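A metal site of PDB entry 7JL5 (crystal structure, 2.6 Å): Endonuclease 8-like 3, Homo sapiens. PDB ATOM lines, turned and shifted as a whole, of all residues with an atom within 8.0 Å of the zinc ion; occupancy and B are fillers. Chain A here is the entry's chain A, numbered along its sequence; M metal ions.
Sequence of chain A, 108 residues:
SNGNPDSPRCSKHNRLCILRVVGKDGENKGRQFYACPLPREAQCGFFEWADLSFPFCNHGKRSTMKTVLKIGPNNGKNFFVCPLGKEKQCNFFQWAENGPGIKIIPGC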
ATOM      1  N   ARG A   9      14.771  20.754  -1.788  1.00  0.00           N
ATOM      2  CA  ARG A   9      14.485  21.349  -0.499  1.00  0.00           C
ATOM      3  C   ARG A   9      15.773  21.934   0.073  1.00  0.00           C
ATOM      4  O   ARG A   9      16.847  21.363  -0.109  1.00  0.00           O
ATOM      5  CB  ARG A   9      13.923  20.306   0.478  1.00  0.00           C
ATOM      6  CG  ARG A   9      12.832  19.434  -0.114  1.00  0.00           C
ATOM      7  CD  ARG A   9      12.537  18.232   0.774  1.00  0.00           C
ATOM      8  NE  ARG A   9      11.316  17.556   0.368  1.00  0.00           N
ATOM      9  CZ  ARG A   9      10.105  17.851   0.857  1.00  0.00           C
ATOM     10  NH1 ARG A   9       9.983  18.797   1.766  1.00  0.00           N
ATOM     11  NH2 ARG A   9       9.037  17.181   0.441  1.00  0.00           N
ATOM     12  N   CYS A  10      15.648  23.074   0.760  1.00  0.00           N
ATOM     13  CA  CYS A  10      16.816  23.591   1.460  1.00  0.00           C
ATOM     14  C   CYS A  10      17.293  22.564   2.489  1.00  0.00           C
ATOM     15  O   CYS A  10      16.597  21.601   2.811  1.00  0.00           O
ATOM     16  CB  CYS A  10      16.491  24.937   2.108  1.00  0.00           C
ATOM     17  SG  CYS A  10      15.006  24.973   3.129  1.00  0.00           S
ATOM     18  N   SER A  11      18.504  22.783   2.995  1.00  0.00           N
ATOM     19  CA  SER A  11      19.127  21.807   3.879  1.00  0.00           C
ATOM     20  C   SER A  11      18.821  22.093   5.347  1.00  0.00           C
ATOM     21  O   SER A  11      18.439  21.170   6.088  1.00  0.00           O
ATOM     22  CB  SER A  11      20.642  21.806   3.650  1.00  0.00           C
ATOM     23  OG  SER A  11      21.116  23.098   3.337  1.00  0.00           O
ATOM     24  N   LYS A  12      18.966  23.338   5.783  1.00  0.00           N
ATOM     25  CA  LYS A  12      18.640  23.691   7.160  1.00  0.00           C
ATOM     26  C   LYS A  12      17.220  23.257   7.498  1.00  0.00           C
ATOM     27  O   LYS A  12      16.991  22.554   8.497  1.00  0.00           O
ATOM     28  CB  LYS A  12      18.819  25.193   7.368  1.00  0.00           C
ATOM     29  N   HIS A  13      16.251  23.679   6.696  1.00  0.00           N
ATOM     30  CA  HIS A  13      14.877  23.220   6.798  1.00  0.00           C
ATOM     31  C   HIS A  13      14.617  22.260   5.646  1.00  0.00           C
ATOM     32  O   HIS A  13      15.063  22.505   4.514  1.00  0.00           O
ATOM     33  CB  HIS A  13      13.893  24.385   6.751  1.00  0.00           C
ATOM     34  CG  HIS A  13      14.460  25.678   7.256  1.00  0.00           C
ATOM     35  ND1 HIS A  13      14.570  26.796   6.470  1.00  0.00           N
ATOM     36  CD2 HIS A  13      14.962  26.012   8.464  1.00  0.00           C
ATOM     37  CE1 HIS A  13      15.110  27.776   7.173  1.00  0.00           C
ATOM     38  NE2 HIS A  13      15.357  27.329   8.387  1.00  0.00           N
ATOM     39  N   ASN A  14      13.901  21.174   5.916  1.00  0.00           N
ATOM     40  CA  ASN A  14      13.612  20.182   4.878  1.00  0.00           C
ATOM     41  C   ASN A  14      12.314  20.539   4.165  1.00  0.00           C
ATOM     42  O   ASN A  14      11.357  19.770   4.124  1.00  0.00           O
ATOM     43  CB  ASN A  14      13.560  18.792   5.491  1.00  0.00           C
ATOM     44  CG  ASN A  14      13.665  17.696   4.461  1.00  0.00           C
ATOM     45  OD1 ASN A  14      12.736  16.930   4.246  1.00  0.00           O
ATOM     46  ND2 ASN A  14      14.816  17.615   3.799  1.00  0.00           N
ATOM     47  N   ARG A  15      12.300  21.740   3.568  1.00  0.00           N
ATOM     48  CA  ARG A  15      11.093  22.324   3.017  1.00  0.00           C
ATOM     49  C   ARG A  15      11.260  22.609   1.527  1.00  0.00           C
ATOM     50  O   ARG A  15      12.338  22.995   1.073  1.00  0.00           O
ATOM     51  CB  ARG A  15      10.731  23.608   3.769  1.00  0.00           C
ATOM     52  CG  ARG A  15      10.461  23.372   5.255  1.00  0.00           C
ATOM     53  CD  ARG A  15       9.839  24.595   5.926  1.00  0.00           C
ATOM     54  NE  ARG A  15       8.398  24.444   6.107  1.00  0.00           N
ATOM     55  CZ  ARG A  15       7.476  24.906   5.265  1.00  0.00           C
ATOM     56  NH1 ARG A  15       7.824  25.551   4.157  1.00  0.00           N
ATOM     57  NH2 ARG A  15       6.193  24.722   5.538  1.00  0.00           N
ATOM     58  N   LEU A  16      10.165  22.428   0.779  1.00  0.00           N
ATOM     59  CA  LEU A  16      10.215  22.549  -0.666  1.00  0.00           C
ATOM     60  C   LEU A  16      10.513  23.981  -1.098  1.00  0.00           C
ATOM     61  O   LEU A  16       9.846  24.923  -0.671  1.00  0.00           O
ATOM     62  CB  LEU A  16       8.884  22.103  -1.279  1.00  0.00           C
ATOM     63  CG  LEU A  16       8.763  20.624  -1.656  1.00  0.00           C
ATOM     64  CD1 LEU A  16       7.351  20.318  -2.108  1.00  0.00           C
ATOM     65  CD2 LEU A  16       9.763  20.263  -2.748  1.00  0.00           C
ATOM     66  N   CYS A  17      11.519  24.127  -1.959  1.00  0.00           N
ATOM     67  CA  CYS A  17      11.974  25.448  -2.370  1.00  0.00           C
ATOM     68  C   CYS A  17      10.965  26.133  -3.274  1.00  0.00           C
ATOM     69  O   CYS A  17      10.171  25.491  -3.966  1.00  0.00           O
ATOM     70  CB  CYS A  17      13.312  25.341  -3.090  1.00  0.00           C
ATOM     71  SG  CYS A  17      14.661  24.688  -2.095  1.00  0.00           S
ATOM     72  N   ALA A  35      15.055  28.612  -4.017  1.00  0.00           N
ATOM     73  CA  ALA A  35      15.429  29.297  -2.795  1.00  0.00           C
ATOM     74  C   ALA A  35      14.500  28.847  -1.665  1.00  0.00           C
ATOM     75  O   ALA A  35      13.473  28.203  -1.890  1.00  0.00           O
ATOM     76  CB  ALA A  35      15.355  30.822  -2.961  1.00  0.00           C
ATOM     77  N   CYS A  36      14.884  29.227  -0.446  1.00  0.00           N
ATOM     78  CA  CYS A  36      14.122  28.834   0.731  1.00  0.00           C
ATOM     79  C   CYS A  36      12.688  29.348   0.626  1.00  0.00           C
ATOM     80  O   CYS A  36      12.455  30.468   0.163  1.00  0.00           O
ATOM     81  CB  CYS A  36      14.792  29.375   1.995  1.00  0.00           C
ATOM     82  SG  CYS A  36      14.107  28.772   3.544  1.00  0.00           S
ATOM     83  N   PRO A  37      11.698  28.562   1.054  1.00  0.00           N
ATOM     84  CA  PRO A  37      10.292  28.971   0.917  1.00  0.00           C
ATOM     85  C   PRO A  37       9.721  29.777   2.072  1.00  0.00           C
ATOM     86  O   PRO A  37       8.586  30.260   1.957  1.00  0.00           O
ATOM     87  CB  PRO A  37       9.558  27.630   0.807  1.00  0.00           C
ATOM     88  CG  PRO A  37      10.376  26.720   1.686  1.00  0.00           C
ATOM     89  CD  PRO A  37      11.813  27.164   1.518  1.00  0.00           C
ATOM     90  N   LEU A  38      10.456  29.945   3.167  1.00  0.00           N
ATOM     91  CA  LEU A  38       9.923  30.604   4.351  1.00  0.00           C
ATOM     92  C   LEU A  38       9.910  32.116   4.159  1.00  0.00           C
ATOM     93  O   LEU A  38      10.462  32.639   3.184  1.00  0.00           O
ATOM     94  CB  LEU A  38      10.763  30.222   5.568  1.00  0.00           C
ATOM     95  CG  LEU A  38      10.927  28.724   5.814  1.00  0.00           C
ATOM     96  CD1 LEU A  38      11.631  28.462   7.136  1.00  0.00           C
ATOM     97  CD2 LEU A  38       9.584  28.008   5.767  1.00  0.00           C
ATOM     98  N   ALA A  42      14.094  34.225   8.899  1.00  0.00           N
ATOM     99  CA  ALA A  42      14.265  32.802   9.130  1.00  0.00           C
ATOM    100  C   ALA A  42      14.652  32.087   7.842  1.00  0.00           C
ATOM    101  O   ALA A  42      15.164  30.962   7.884  1.00  0.00           O
ATOM    102  CB  ALA A  42      13.002  32.179   9.732  1.00  0.00           C
ATOM    103  N   GLN A  43      14.397  32.723   6.705  1.00  0.00           N
ATOM    104  CA  GLN A  43      14.864  32.203   5.419  1.00  0.00           C
ATOM    105  C   GLN A  43      16.333  31.836   5.501  1.00  0.00           C
ATOM    106  O   GLN A  43      17.174  32.675   5.860  1.00  0.00           O
ATOM    107  CB  GLN A  43      14.644  33.239   4.320  1.00  0.00           C
ATOM    108  CG  GLN A  43      13.522  32.916   3.351  1.00  0.00           C
ATOM    109  CD  GLN A  43      13.520  33.854   2.157  1.00  0.00           C
ATOM    110  OE1 GLN A  43      14.566  34.364   1.748  1.00  0.00           O
ATOM    111  NE2 GLN A  43      12.337  34.095   1.590  1.00  0.00           N
ATOM    112  N   CYS A  44      16.659  30.593   5.175  1.00  0.00           N
ATOM    113  CA  CYS A  44      18.057  30.211   5.056  1.00  0.00           C
ATOM    114  C   CYS A  44      18.633  30.775   3.763  1.00  0.00           C
ATOM    115  O   CYS A  44      17.917  31.270   2.880  1.00  0.00           O
ATOM    116  CB  CYS A  44      18.220  28.698   5.116  1.00  0.00           C
ATOM    117  SG  CYS A  44      17.374  27.796   3.795  1.00  0.00           S
ATOM    118  N   GLY A  45      19.952  30.708   3.636  1.00  0.00           N
ATOM    119  CA  GLY A  45      20.619  31.258   2.480  1.00  0.00           C
ATOM    120  C   GLY A  45      20.681  30.299   1.311  1.00  0.00           C
ATOM    121  O   GLY A  45      21.551  30.433   0.444  1.00  0.00           O
ATOM    122  N   PHE A  46      19.761  29.329   1.264  1.00  0.00           N
ATOM    123  CA  PHE A  46      19.784  28.338   0.205  1.00  0.00           C
ATOM    124  C   PHE A  46      19.669  29.029  -1.152  1.00  0.00           C
ATOM    125  O   PHE A  46      19.003  30.051  -1.311  1.00  0.00           O
ATOM    126  CB  PHE A  46      18.631  27.342   0.374  1.00  0.00           C
ATOM    127  CG  PHE A  46      18.769  26.113  -0.488  1.00  0.00           C
ATOM    128  CD1 PHE A  46      19.567  25.055  -0.065  1.00  0.00           C
ATOM    129  CD2 PHE A  46      18.107  26.019  -1.694  1.00  0.00           C
ATOM    130  CE1 PHE A  46      19.692  23.923  -0.848  1.00  0.00           C
ATOM    131  CE2 PHE A  46      18.245  24.889  -2.483  1.00  0.00           C
ATOM    132  CZ  PHE A  46      19.029  23.839  -2.052  1.00  0.00           C
HETATM  133 ZN    ZN M   1      15.365  26.869   4.348  1.00  0.00          ZN
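Of the 18 residues printed, 4 come within 4 Å of the zinc ion.
The zinc ion is bound by a ring nitrogen (ND1) of His 13 (2.3 Å), the side-chain sulfur of Cys 44 (2.3 Å), the side-chain sulfur of Cys 10 (2.3 Å) and the side-chain sulfur of Cys 36 (2.4 Å).
N of Cys 10 is in hydrogen-bond range of O of Arg 15, 3.3 Å away.
SG of Cys 17 is in hydrogen-bond range of N of Cys 10, at 3.4 Å.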
